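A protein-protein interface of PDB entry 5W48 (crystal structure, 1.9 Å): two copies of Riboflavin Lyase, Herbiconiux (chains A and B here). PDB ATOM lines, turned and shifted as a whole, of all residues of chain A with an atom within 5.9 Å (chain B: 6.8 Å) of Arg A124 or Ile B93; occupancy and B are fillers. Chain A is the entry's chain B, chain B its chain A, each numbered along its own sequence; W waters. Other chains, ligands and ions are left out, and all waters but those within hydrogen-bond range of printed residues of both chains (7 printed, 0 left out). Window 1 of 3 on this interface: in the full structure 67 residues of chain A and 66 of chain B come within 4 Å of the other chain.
Water W1 lies within hydrogen-bond range of the side-chain carboxylate (OD1) of Asp B90 and the guanidinium group (NE) of Arg A124.
Water W5 lies within hydrogen-bond range of O of Ala A96 (2.6 Å), O of Ala B97 (3.1 Å) and N of Ile A99 (3.4 Å).
Water W7 lies within hydrogen-bond range of O of Ser A120 (2.8 Å), NE of Arg A123 (3.0 Å), N of Arg A124 (3.3 Å) and OD2 of Asp B90 (3.4 Å).
Water W6 lies within hydrogen-bond range of OD1 of Asp A90 (2.8 Å) and NH2 of Arg B124 (3.5 Å).
The guanidinium group (NH2) of Arg A123 lies within salt-bridge range of the side-chain carboxylate (OD2) of Asp B90.
The side-chain hydroxyl of Ser A127 is in hydrogen-bond range of the backbone NH of Asp B90, 2.9 Å away.
The guanidinium group (NH2) of Arg B124 lies close to the guanidinium group (NH2) of Arg A124 (3.0 Å).
Of the 19 printed residues of chain B, 10 touch a printed residue of chain A.
Printed residues of chain B that touch a printed residue of chain A: Leu B42, Trp B66, Leu B89, Asp B90, Pro B91, Ile B93, Ala B96, Ala B97, Arg B124 and Leu B128.
Hydrophobic or aromatic side chains of chain B that line the printed part of chain A: Leu B42, Trp B66, Leu B89, Pro B91, Ile B93, Ala B96, Ala B97 and Leu B128.
Among the printed residues, Asp or Glu carboxylates within 4 Å of a Lys or Arg side-chain nitrogen of the other chain: Arg A123 with Asp B90 (3.0 Å).
The guanidinium group (NH1) of Arg B124 lies within salt-bridge range of the side-chain carboxylate (OE1) of Glu B116 (3.1 Å).
The side-chain carboxylate (OD2) of Asp A90 sits at hydrogen-bond distance from the backbone NH (N) of Ile A93 (3.2 Å).
The side-chain carboxylate of Glu A116 is in salt-bridge range of the guanidinium group of Arg A124 (3.0 Å).
The side-chain hydroxyl of Ser A127 lies within hydrogen-bond range of the backbone carbonyl oxygen of Arg A123, at 2.7 Å.
Ile A93 touches Ala B96, and with the chains exchanged Ala A96 touches Ile B93.
Ile A93 touches Arg B124, and with the chains exchanged Arg A124 touches Ile B93.
Arg A124 touches Asp B90, but with the chains exchanged Asp A90 does not touch Arg B124 (4.2 Å).
Arg A124 touches its own counterpart, Arg B124.
Of the 20 pairs that touch across the chains among the printed residues, 8 have their exchanged pair printed and touching as well.
Among the printed residues, pairs that only touch across the chains: Ile A93 with Ala B96 (3.8 Å), Ile A93 with Arg B124 (3.7 Å), Ile A93 with Leu B128 (3.98 Å), Ala A96 with Ile B93 (3.8 Å), Ala A96 with Ala B96 (3.4 Å), Ala A96 with Ala B97 (3.5 Å), Ile A99 with Leu B42 (3.7 Å), Ser A120 with Trp B66 (3.4 Å), Arg A123 with Trp B66 (3.2 Å), Arg A123 with Pro B91 (3.6 Å), Arg A124 with Asp B90 (3.9 Å), Arg A124 with Ile B93 (3.8 Å), Ser A127 with Leu B89 (3.5 Å), Leu A128 with Ile B93 (3.9 Å), Leu A131 with Leu B42 (3.7 Å), Leu A131 with Leu B89 (3.9 Å) and Leu A131 with Ile B93 (3.9 Å).
Of the printed residues of chain B, Ile A99 touches Leu B42 (3.7 Å).
Arg A124 touches just these residues of chain B: Asp B90 (3.9 Å), Ile B93 (3.8 Å) and Arg B124 (3.0 Å).
Printed residues of chain A within 4 Å of Leu B42: Ile A99 and Leu A131.
Of the printed residues of chain A, Ile B93 touches Ala A96 (3.8 Å), Arg A124 (3.8 Å), Leu A128 (3.9 Å) and Leu A131 (3.9 Å).
Of the printed residues of chain A, Ala B96 touches Ile A93 and Ala A96.
The nearest residue of chain B that does not touch Arg A124 is Glu B116 (5.1 Å).
The nearest printed residue of chain A that does not touch Ile B93 is Ser A127 (4.1 Å).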
ATOM      1  N   ASP A  90      25.702  -8.249  19.816  1.00  0.00           N
ATOM      2  CA  ASP A  90      26.667  -8.173  18.726  1.00  0.00           C
ATOM      3  C   ASP A  90      27.283  -6.774  18.643  1.00  0.00           C
ATOM      4  O   ASP A  90      26.545  -5.788  18.516  1.00  0.00           O
ATOM      5  CB  ASP A  90      25.998  -8.523  17.408  1.00  0.00           C
ATOM      6  CG  ASP A  90      26.968  -8.450  16.236  1.00  0.00           C
ATOM      7  OD1 ASP A  90      27.809  -9.363  16.082  1.00  0.00           O
ATOM      8  OD2 ASP A  90      26.905  -7.468  15.477  1.00  0.00           O
ATOM      9  N   ALA A  92      29.017  -5.162  16.248  1.00  0.00           N
ATOM     10  CA  ALA A  92      28.790  -4.408  15.009  1.00  0.00           C
ATOM     11  C   ALA A  92      27.441  -3.693  15.018  1.00  0.00           C
ATOM     12  O   ALA A  92      27.295  -2.610  14.428  1.00  0.00           O
ATOM     13  CB  ALA A  92      28.874  -5.328  13.792  1.00  0.00           C
ATOM     14  N   ILE A  93      26.441  -4.284  15.668  1.00  0.00           N
ATOM     15  CA  ILE A  93      25.130  -3.652  15.738  1.00  0.00           C
ATOM     16  C   ILE A  93      25.154  -2.484  16.713  1.00  0.00           C
ATOM     17  O   ILE A  93      24.574  -1.420  16.446  1.00  0.00           O
ATOM     18  CB  ILE A  93      24.066  -4.700  16.120  1.00  0.00           C
ATOM     19  CG1 ILE A  93      23.932  -5.758  15.005  1.00  0.00           C
ATOM     20  CG2 ILE A  93      22.745  -4.025  16.492  1.00  0.00           C
ATOM     21  CD1 ILE A  93      23.542  -5.192  13.623  1.00  0.00           C
ATOM     22  N   ALA A  96      27.031   0.395  14.840  1.00  0.00           N
ATOM     23  CA  ALA A  96      26.169   1.053  13.858  1.00  0.00           C
ATOM     24  C   ALA A  96      25.163   1.984  14.532  1.00  0.00           C
ATOM     25  O   ALA A  96      24.956   3.121  14.081  1.00  0.00           O
ATOM     26  CB  ALA A  96      25.450  -0.001  13.005  1.00  0.00           C
ATOM     27  N   ILE A  99      26.534   5.430  15.414  1.00  0.00           N
ATOM     28  CA  ILE A  99      26.929   6.348  14.345  1.00  0.00           C
ATOM     29  C   ILE A  99      26.068   7.598  14.363  1.00  0.00           C
ATOM     30  O   ILE A  99      26.579   8.716  14.231  1.00  0.00           O
ATOM     31  CB  ILE A  99      26.867   5.637  12.981  1.00  0.00           C
ATOM     32  CG1 ILE A  99      27.968   4.576  12.893  1.00  0.00           C
ATOM     33  CG2 ILE A  99      26.989   6.655  11.827  1.00  0.00           C
ATOM     34  CD1 ILE A  99      27.901   3.729  11.619  1.00  0.00           C
ATOM     35  N   GLU A 116      34.473 -15.430  11.154  1.00  0.00           N
ATOM     36  CA  GLU A 116      33.804 -14.629  10.134  1.00  0.00           C
ATOM     37  C   GLU A 116      34.047 -15.200   8.732  1.00  0.00           C
ATOM     38  O   GLU A 116      35.086 -15.799   8.443  1.00  0.00           O
ATOM     39  CB  GLU A 116      34.289 -13.166  10.185  1.00  0.00           C
ATOM     40  CG  GLU A 116      33.965 -12.421  11.480  1.00  0.00           C
ATOM     41  CD  GLU A 116      32.520 -11.938  11.559  1.00  0.00           C
ATOM     42  OE1 GLU A 116      31.826 -11.975  10.519  1.00  0.00           O
ATOM     43  OE2 GLU A 116      32.083 -11.509  12.656  1.00  0.00           O
ATOM     44  N   TYR A 119      34.024 -12.421   2.960  1.00  0.00           N
ATOM     45  CA  TYR A 119      33.297 -11.621   1.972  1.00  0.00           C
ATOM     46  C   TYR A 119      32.178 -10.806   2.618  1.00  0.00           C
ATOM     47  O   TYR A 119      32.001  -9.619   2.308  1.00  0.00           O
ATOM     48  CB  TYR A 119      32.739 -12.521   0.872  1.00  0.00           C
ATOM     49  CG  TYR A 119      32.228 -11.740  -0.327  1.00  0.00           C
ATOM     50  CD1 TYR A 119      33.086 -11.376  -1.366  1.00  0.00           C
ATOM     51  CD2 TYR A 119      30.899 -11.357  -0.415  1.00  0.00           C
ATOM     52  CE1 TYR A 119      32.619 -10.667  -2.469  1.00  0.00           C
ATOM     53  CE2 TYR A 119      30.430 -10.638  -1.515  1.00  0.00           C
ATOM     54  CZ  TYR A 119      31.302 -10.300  -2.533  1.00  0.00           C
ATOM     55  OH  TYR A 119      30.838  -9.600  -3.632  1.00  0.00           O
ATOM     56  N   SER A 120      31.415 -11.416   3.525  1.00  0.00           N
ATOM     57  CA  SER A 120      30.337 -10.684   4.176  1.00  0.00           C
ATOM     58  C   SER A 120      30.864  -9.750   5.255  1.00  0.00           C
ATOM     59  O   SER A 120      30.289  -8.679   5.474  1.00  0.00           O
ATOM     60  CB  SER A 120      29.299 -11.660   4.749  1.00  0.00           C
ATOM     61  OG  SER A 120      29.893 -12.606   5.607  1.00  0.00           O
ATOM     62  N   PHE A 121      31.960 -10.130   5.914  1.00  0.00           N
ATOM     63  CA  PHE A 121      32.602  -9.244   6.881  1.00  0.00           C
ATOM     64  C   PHE A 121      33.129  -7.982   6.205  1.00  0.00           C
ATOM     65  O   PHE A 121      32.964  -6.871   6.723  1.00  0.00           O
ATOM     66  CB  PHE A 121      33.743  -9.993   7.579  1.00  0.00           C
ATOM     67  CG  PHE A 121      34.478  -9.169   8.591  1.00  0.00           C
ATOM     68  CD1 PHE A 121      33.911  -8.911   9.836  1.00  0.00           C
ATOM     69  CD2 PHE A 121      35.718  -8.635   8.299  1.00  0.00           C
ATOM     70  CE1 PHE A 121      34.568  -8.118  10.770  1.00  0.00           C
ATOM     71  CE2 PHE A 121      36.394  -7.861   9.233  1.00  0.00           C
ATOM     72  CZ  PHE A 121      35.821  -7.608  10.470  1.00  0.00           C
ATOM     73  N   ALA A 122      33.782  -8.138   5.057  1.00  0.00           N
ATOM     74  CA  ALA A 122      34.312  -6.974   4.354  1.00  0.00           C
ATOM     75  C   ALA A 122      33.196  -5.999   4.004  1.00  0.00           C
ATOM     76  O   ALA A 122      33.346  -4.786   4.182  1.00  0.00           O
ATOM     77  CB  ALA A 122      35.044  -7.417   3.092  1.00  0.00           C
ATOM     78  N   ARG A 123      32.066  -6.522   3.525  1.00  0.00           N
ATOM     79  CA  ARG A 123      30.915  -5.686   3.190  1.00  0.00           C
ATOM     80  C   ARG A 123      30.324  -5.024   4.426  1.00  0.00           C
ATOM     81  O   ARG A 123      29.932  -3.852   4.383  1.00  0.00           O
ATOM     82  CB  ARG A 123      29.846  -6.521   2.488  1.00  0.00           C
ATOM     83  CG  ARG A 123      28.656  -5.669   2.024  1.00  0.00           C
ATOM     84  CD  ARG A 123      27.580  -6.468   1.318  1.00  0.00           C
ATOM     85  NE  ARG A 123      26.577  -7.016   2.241  1.00  0.00           N
ATOM     86  CZ  ARG A 123      25.357  -7.400   1.864  1.00  0.00           C
ATOM     87  NH1 ARG A 123      24.979  -7.287   0.585  1.00  0.00           N
ATOM     88  NH2 ARG A 123      24.505  -7.883   2.759  1.00  0.00           N
ATOM     89  N   ARG A 124      30.237  -5.764   5.531  1.00  0.00           N
ATOM     90  CA  ARG A 124      29.715  -5.197   6.767  1.00  0.00           C
ATOM     91  C   ARG A 124      30.591  -4.051   7.260  1.00  0.00           C
ATOM     92  O   ARG A 124      30.087  -2.977   7.619  1.00  0.00           O
ATOM     93  CB  ARG A 124      29.610  -6.298   7.836  1.00  0.00           C
ATOM     94  CG  ARG A 124      28.914  -5.849   9.119  1.00  0.00           C
ATOM     95  CD  ARG A 124      28.817  -7.025  10.139  1.00  0.00           C
ATOM     96  NE  ARG A 124      28.266  -8.213   9.496  1.00  0.00           N
ATOM     97  CZ  ARG A 124      28.863  -9.402   9.467  1.00  0.00           C
ATOM     98  NH1 ARG A 124      30.019  -9.588  10.093  1.00  0.00           N
ATOM     99  NH2 ARG A 124      28.285 -10.414   8.828  1.00  0.00           N
ATOM    100  N   MET A 125      31.912  -4.258   7.282  1.00  0.00           N
ATOM    101  CA  MET A 125      32.812  -3.222   7.795  1.00  0.00           C
ATOM    102  C   MET A 125      32.870  -2.007   6.875  1.00  0.00           C
ATOM    103  O   MET A 125      32.959  -0.871   7.354  1.00  0.00           O
ATOM    104  CB  MET A 125      34.223  -3.789   8.010  1.00  0.00           C
ATOM    105  CG  MET A 125      34.283  -4.886   9.072  1.00  0.00           C
ATOM    106  SD  MET A 125      33.634  -4.370  10.689  1.00  0.00           S
ATOM    107  CE  MET A 125      34.966  -3.296  11.199  1.00  0.00           C
ATOM    108  N   ALA A 126      32.859  -2.220   5.557  1.00  0.00           N
ATOM    109  CA  ALA A 126      32.888  -1.089   4.633  1.00  0.00           C
ATOM    110  C   ALA A 126      31.594  -0.288   4.702  1.00  0.00           C
ATOM    111  O   ALA A 126      31.604   0.938   4.508  1.00  0.00           O
ATOM    112  CB  ALA A 126      33.163  -1.593   3.208  1.00  0.00           C
ATOM    113  N   SER A 127      30.479  -0.956   5.001  1.00  0.00           N
ATOM    114  CA  SER A 127      29.209  -0.269   5.196  1.00  0.00           C
ATOM    115  C   SER A 127      29.234   0.601   6.447  1.00  0.00           C
ATOM    116  O   SER A 127      28.697   1.713   6.443  1.00  0.00           O
ATOM    117  CB  SER A 127      28.057  -1.284   5.297  1.00  0.00           C
ATOM    118  OG  SER A 127      27.897  -2.045   4.110  1.00  0.00           O
ATOM    119  N   LEU A 128      29.784   0.085   7.551  1.00  0.00           N
ATOM    120  CA  LEU A 128      30.005   0.934   8.721  1.00  0.00           C
ATOM    121  C   LEU A 128      30.882   2.131   8.376  1.00  0.00           C
ATOM    122  O   LEU A 128      30.608   3.257   8.813  1.00  0.00           O
ATOM    123  CB  LEU A 128      30.659   0.133   9.852  1.00  0.00           C
ATOM    124  CG  LEU A 128      29.769  -0.874  10.566  1.00  0.00           C
ATOM    125  CD1 LEU A 128      30.638  -1.917  11.296  1.00  0.00           C
ATOM    126  CD2 LEU A 128      28.914  -0.123  11.547  1.00  0.00           C
ATOM    127  N   ASP A 129      31.947   1.901   7.595  1.00  0.00           N
ATOM    128  CA  ASP A 129      32.866   2.982   7.241  1.00  0.00           C
ATOM    129  C   ASP A 129      32.200   4.040   6.357  1.00  0.00           C
ATOM    130  O   ASP A 129      32.406   5.243   6.567  1.00  0.00           O
ATOM    131  CB  ASP A 129      34.109   2.400   6.564  1.00  0.00           C
ATOM    132  CG  ASP A 129      35.302   3.346   6.624  1.00  0.00           C
ATOM    133  OD1 ASP A 129      35.688   3.762   7.745  1.00  0.00           O
ATOM    134  OD2 ASP A 129      35.847   3.686   5.552  1.00  0.00           O
ATOM    135  N   LEU A 131      28.863   4.771   6.250  1.00  0.00           N
ATOM    136  CA  LEU A 131      27.849   5.511   6.994  1.00  0.00           C
ATOM    137  C   LEU A 131      28.457   6.397   8.075  1.00  0.00           C
ATOM    138  O   LEU A 131      27.883   7.444   8.395  1.00  0.00           O
ATOM    139  CB  LEU A 131      26.833   4.555   7.617  1.00  0.00           C
ATOM    140  CG  LEU A 131      25.919   3.793   6.639  1.00  0.00           C
ATOM    141  CD1 LEU A 131      24.916   2.907   7.407  1.00  0.00           C
ATOM    142  CD2 LEU A 131      25.182   4.747   5.711  1.00  0.00           C
ATOM    143  N   THR A 219      30.805  -3.593  -2.008  1.00  0.00           N
ATOM    144  CA  THR A 219      30.907  -2.200  -1.588  1.00  0.00           C
ATOM    145  C   THR A 219      32.043  -1.496  -2.313  1.00  0.00           C
ATOM    146  O   THR A 219      33.123  -2.059  -2.497  1.00  0.00           O
ATOM    147  CB  THR A 219      31.136  -2.089  -0.081  1.00  0.00           C
ATOM    148  OG1 THR A 219      32.326  -2.818   0.270  1.00  0.00           O
ATOM    149  CG2 THR A 219      29.929  -2.651   0.681  1.00  0.00           C
ATOM    150  N   LEU B  42      24.446   8.336   5.454  1.00  0.00           N
ATOM    151  CA  LEU B  42      23.425   8.117   6.475  1.00  0.00           C
ATOM    152  C   LEU B  42      22.287   9.122   6.350  1.00  0.00           C
ATOM    153  O   LEU B  42      21.132   8.791   6.646  1.00  0.00           O
ATOM    154  CB  LEU B  42      24.047   8.193   7.868  1.00  0.00           C
ATOM    155  CG  LEU B  42      23.087   7.799   8.999  1.00  0.00           C
ATOM    156  CD1 LEU B  42      22.414   6.439   8.756  1.00  0.00           C
ATOM    157  CD2 LEU B  42      23.862   7.784  10.293  1.00  0.00           C
ATOM    158  N   LEU B  62      14.207  -3.166   3.961  1.00  0.00           N
ATOM    159  CA  LEU B  62      15.455  -3.114   3.207  1.00  0.00           C
ATOM    160  C   LEU B  62      15.675  -4.447   2.498  1.00  0.00           C
ATOM    161  O   LEU B  62      15.979  -5.454   3.145  1.00  0.00           O
ATOM    162  CB  LEU B  62      16.622  -2.813   4.148  1.00  0.00           C
ATOM    163  CG  LEU B  62      16.500  -1.496   4.912  1.00  0.00           C
ATOM    164  CD1 LEU B  62      17.617  -1.350   5.919  1.00  0.00           C
ATOM    165  CD2 LEU B  62      16.518  -0.354   3.920  1.00  0.00           C
ATOM    166  N   TRP B  66      23.473 -10.277  -2.952  1.00  0.00           N
ATOM    167  CA  TRP B  66      24.883 -10.580  -2.773  1.00  0.00           C
ATOM    168  C   TRP B  66      25.657 -10.637  -4.076  1.00  0.00           C
ATOM    169  O   TRP B  66      26.874 -10.437  -4.054  1.00  0.00           O
ATOM    170  CB  TRP B  66      25.058 -11.916  -2.033  1.00  0.00           C
ATOM    171  CG  TRP B  66      24.770 -11.833  -0.574  1.00  0.00           C
ATOM    172  CD1 TRP B  66      23.638 -12.249   0.072  1.00  0.00           C
ATOM    173  CD2 TRP B  66      25.624 -11.280   0.430  1.00  0.00           C
ATOM    174  NE1 TRP B  66      23.746 -12.004   1.416  1.00  0.00           N
ATOM    175  CE2 TRP B  66      24.952 -11.407   1.665  1.00  0.00           C
ATOM    176  CE3 TRP B  66      26.890 -10.681   0.402  1.00  0.00           C
ATOM    177  CZ2 TRP B  66      25.505 -10.965   2.871  1.00  0.00           C
ATOM    178  CZ3 TRP B  66      27.443 -10.245   1.604  1.00  0.00           C
ATOM    179  CH2 TRP B  66      26.745 -10.396   2.825  1.00  0.00           C
ATOM    180  N   LEU B  89      25.157  -1.452   0.129  1.00  0.00           N
ATOM    181  CA  LEU B  89      25.546  -1.584   1.532  1.00  0.00           C
ATOM    182  C   LEU B  89      24.869  -2.789   2.179  1.00  0.00           C
ATOM    183  O   LEU B  89      23.886  -3.333   1.670  1.00  0.00           O
ATOM    184  CB  LEU B  89      25.183  -0.329   2.329  1.00  0.00           C
ATOM    185  CG  LEU B  89      25.775   1.026   1.931  1.00  0.00           C
ATOM    186  CD1 LEU B  89      25.338   2.052   2.958  1.00  0.00           C
ATOM    187  CD2 LEU B  89      27.290   0.987   1.808  1.00  0.00           C
ATOM    188  N   ASP B  90      25.402  -3.184   3.335  1.00  0.00           N
ATOM    189  CA  ASP B  90      24.791  -4.222   4.165  1.00  0.00           C
ATOM    190  C   ASP B  90      23.536  -3.702   4.858  1.00  0.00           C
ATOM    191  O   ASP B  90      23.621  -2.733   5.622  1.00  0.00           O
ATOM    192  CB  ASP B  90      25.801  -4.695   5.210  1.00  0.00           C
ATOM    193  CG  ASP B  90      25.245  -5.831   6.100  1.00  0.00           C
ATOM    194  OD1 ASP B  90      25.503  -5.814   7.318  1.00  0.00           O
ATOM    195  OD2 ASP B  90      24.571  -6.745   5.581  1.00  0.00           O
ATOM    196  N   PRO B  91      22.364  -4.314   4.646  1.00  0.00           N
ATOM    197  CA  PRO B  91      21.134  -3.756   5.242  1.00  0.00           C
ATOM    198  C   PRO B  91      21.074  -3.831   6.762  1.00  0.00           C
ATOM    199  O   PRO B  91      20.415  -2.982   7.378  1.00  0.00           O
ATOM    200  CB  PRO B  91      20.006  -4.578   4.590  1.00  0.00           C
ATOM    201  CG  PRO B  91      20.664  -5.737   3.927  1.00  0.00           C
ATOM    202  CD  PRO B  91      22.080  -5.340   3.627  1.00  0.00           C
ATOM    203  N   ALA B  92      21.720  -4.810   7.402  1.00  0.00           N
ATOM    204  CA  ALA B  92      21.663  -4.861   8.862  1.00  0.00           C
ATOM    205  C   ALA B  92      22.334  -3.630   9.470  1.00  0.00           C
ATOM    206  O   ALA B  92      21.880  -3.103  10.494  1.00  0.00           O
ATOM    207  CB  ALA B  92      22.309  -6.150   9.383  1.00  0.00           C
ATOM    208  N   ILE B  93      23.412  -3.156   8.841  1.00  0.00           N
ATOM    209  CA  ILE B  93      24.101  -1.956   9.307  1.00  0.00           C
ATOM    210  C   ILE B  93      23.215  -0.725   9.127  1.00  0.00           C
ATOM    211  O   ILE B  93      23.068   0.092  10.043  1.00  0.00           O
ATOM    212  CB  ILE B  93      25.445  -1.811   8.567  1.00  0.00           C
ATOM    213  CG1 ILE B  93      26.367  -2.990   8.915  1.00  0.00           C
ATOM    214  CG2 ILE B  93      26.101  -0.468   8.888  1.00  0.00           C
ATOM    215  CD1 ILE B  93      26.532  -3.217  10.417  1.00  0.00           C
ATOM    216  N   VAL B  94      22.601  -0.577   7.945  1.00  0.00           N
ATOM    217  CA  VAL B  94      21.648   0.515   7.734  1.00  0.00           C
ATOM    218  C   VAL B  94      20.538   0.441   8.775  1.00  0.00           C
ATOM    219  O   VAL B  94      20.183   1.444   9.404  1.00  0.00           O
ATOM    220  CB  VAL B  94      21.080   0.480   6.296  1.00  0.00           C
ATOM    221  CG1 VAL B  94      20.048   1.609   6.076  1.00  0.00           C
ATOM    222  CG2 VAL B  94      22.188   0.585   5.255  1.00  0.00           C
ATOM    223  N   ALA B  95      19.977  -0.755   8.981  1.00  0.00           N
ATOM    224  CA  ALA B  95      18.886  -0.909   9.940  1.00  0.00           C
ATOM    225  C   ALA B  95      19.329  -0.504  11.340  1.00  0.00           C
ATOM    226  O   ALA B  95      18.614   0.209  12.053  1.00  0.00           O
ATOM    227  CB  ALA B  95      18.372  -2.356   9.938  1.00  0.00           C
ATOM    228  N   ALA B  96      20.518  -0.948  11.749  1.00  0.00           N
ATOM    229  CA  ALA B  96      21.003  -0.600  13.080  1.00  0.00           C
ATOM    230  C   ALA B  96      21.208   0.903  13.218  1.00  0.00           C
ATOM    231  O   ALA B  96      20.878   1.487  14.256  1.00  0.00           O
ATOM    232  CB  ALA B  96      22.302  -1.340  13.374  1.00  0.00           C
ATOM    233  N   ALA B  97      21.720   1.553  12.168  1.00  0.00           N
ATOM    234  CA  ALA B  97      21.928   2.998  12.257  1.00  0.00           C
ATOM    235  C   ALA B  97      20.600   3.741  12.346  1.00  0.00           C
ATOM    236  O   ALA B  97      20.511   4.785  13.005  1.00  0.00           O
ATOM    237  CB  ALA B  97      22.754   3.481  11.060  1.00  0.00           C
ATOM    238  N   LEU B  98      19.550   3.210  11.719  1.00  0.00           N
ATOM    239  CA  LEU B  98      18.243   3.853  11.792  1.00  0.00           C
ATOM    240  C   LEU B  98      17.555   3.671  13.143  1.00  0.00           C
ATOM    241  O   LEU B  98      16.607   4.410  13.441  1.00  0.00           O
ATOM    242  CB  LEU B  98      17.338   3.314  10.690  1.00  0.00           C
ATOM    243  CG  LEU B  98      17.707   3.839   9.309  1.00  0.00           C
ATOM    244  CD1 LEU B  98      16.778   3.241   8.278  1.00  0.00           C
ATOM    245  CD2 LEU B  98      17.638   5.373   9.310  1.00  0.00           C
ATOM    246  N   MET B 109      14.549  -6.355   7.323  1.00  0.00           N
ATOM    247  CA  MET B 109      15.709  -6.546   6.468  1.00  0.00           C
ATOM    248  C   MET B 109      15.737  -7.955   5.915  1.00  0.00           C
ATOM    249  O   MET B 109      15.331  -8.919   6.577  1.00  0.00           O
ATOM    250  CB  MET B 109      17.003  -6.278   7.214  1.00  0.00           C
ATOM    251  CG  MET B 109      16.967  -6.850   8.602  1.00  0.00           C
ATOM    252  SD  MET B 109      18.587  -6.790   9.354  1.00  0.00           S
ATOM    253  CE  MET B 109      19.388  -8.144   8.476  1.00  0.00           C
ATOM    254  N   GLU B 116      24.082 -16.980   5.237  1.00  0.00           N
ATOM    255  CA  GLU B 116      24.339 -16.597   6.625  1.00  0.00           C
ATOM    256  C   GLU B 116      24.690 -17.814   7.478  1.00  0.00           C
ATOM    257  O   GLU B 116      24.213 -18.932   7.236  1.00  0.00           O
ATOM    258  CB  GLU B 116      23.118 -15.899   7.234  1.00  0.00           C
ATOM    259  CG  GLU B 116      22.787 -14.541   6.604  1.00  0.00           C
ATOM    260  CD  GLU B 116      23.699 -13.423   7.084  1.00  0.00           C
ATOM    261  OE1 GLU B 116      24.395 -13.618   8.102  1.00  0.00           O
ATOM    262  OE2 GLU B 116      23.716 -12.346   6.445  1.00  0.00           O
ATOM    263  N   GLN B 117      25.528 -17.587   8.492  1.00  0.00           N
ATOM    264  CA  GLN B 117      25.744 -18.587   9.538  1.00  0.00           C
ATOM    265  C   GLN B 117      24.672 -18.408  10.605  1.00  0.00           C
ATOM    266  O   GLN B 117      24.583 -17.327  11.197  1.00  0.00           O
ATOM    267  CB  GLN B 117      27.133 -18.443  10.160  1.00  0.00           C
ATOM    268  CG  GLN B 117      28.301 -18.476   9.173  1.00  0.00           C
ATOM    269  CD  GLN B 117      29.616 -17.958   9.786  1.00  0.00           C
ATOM    270  OE1 GLN B 117      29.722 -16.791  10.189  1.00  0.00           O
ATOM    271  NE2 GLN B 117      30.617 -18.832   9.858  1.00  0.00           N
ATOM    272  N   SER B 120      25.621 -16.764  14.300  1.00  0.00           N
ATOM    273  CA  SER B 120      25.918 -15.342  14.318  1.00  0.00           C
ATOM    274  C   SER B 120      24.726 -14.525  13.829  1.00  0.00           C
ATOM    275  O   SER B 120      24.517 -13.396  14.287  1.00  0.00           O
ATOM    276  CB  SER B 120      27.169 -15.053  13.478  1.00  0.00           C
ATOM    277  OG  SER B 120      27.077 -15.634  12.184  1.00  0.00           O
ATOM    278  N   ARG B 124      22.856 -11.438  15.859  1.00  0.00           N
ATOM    279  CA  ARG B 124      22.759 -10.117  15.239  1.00  0.00           C
ATOM    280  C   ARG B 124      21.318  -9.611  15.238  1.00  0.00           C
ATOM    281  O   ARG B 124      21.040  -8.487  15.675  1.00  0.00           O
ATOM    282  CB  ARG B 124      23.321 -10.183  13.814  1.00  0.00           C
ATOM    283  CG  ARG B 124      23.407  -8.832  13.097  1.00  0.00           C
ATOM    284  CD  ARG B 124      24.051  -8.965  11.686  1.00  0.00           C
ATOM    285  NE  ARG B 124      25.299  -9.738  11.712  1.00  0.00           N
ATOM    286  CZ  ARG B 124      25.499 -10.854  11.015  1.00  0.00           C
ATOM    287  NH1 ARG B 124      24.556 -11.321  10.203  1.00  0.00           N
ATOM    288  NH2 ARG B 124      26.652 -11.495  11.113  1.00  0.00           N
ATOM    289  N   LEU B 128      19.585  -6.377  17.282  1.00  0.00           N
ATOM    290  CA  LEU B 128      18.719  -5.358  16.690  1.00  0.00           C
ATOM    291  C   LEU B 128      17.393  -5.269  17.435  1.00  0.00           C
ATOM    292  O   LEU B 128      16.867  -4.176  17.642  1.00  0.00           O
ATOM    293  CB  LEU B 128      18.472  -5.670  15.199  1.00  0.00           C
ATOM    294  CG  LEU B 128      19.614  -5.390  14.217  1.00  0.00           C
ATOM    295  CD1 LEU B 128      19.490  -6.261  12.949  1.00  0.00           C
ATOM    296  CD2 LEU B 128      19.572  -3.901  13.842  1.00  0.00           C
HETATM  297  O   HOH W   1      25.794  -7.820   8.708  1.00  0.00           O
HETATM  298  O   HOH W   2      27.142   9.170   6.169  1.00  0.00           O
HETATM  299  O   HOH W   3      27.489  -8.737  12.935  1.00  0.00           O
HETATM  300  O   HOH W   4      26.358 -11.642  15.765  1.00  0.00           O
HETATM  301  O   HOH W   5      23.428   5.246  14.026  1.00  0.00           O
HETATM  302  O   HOH W   6      28.639 -10.916  13.912  1.00  0.00           O
HETATM  303  O   HOH W   7      27.723  -7.814   4.925  1.00  0.00           O
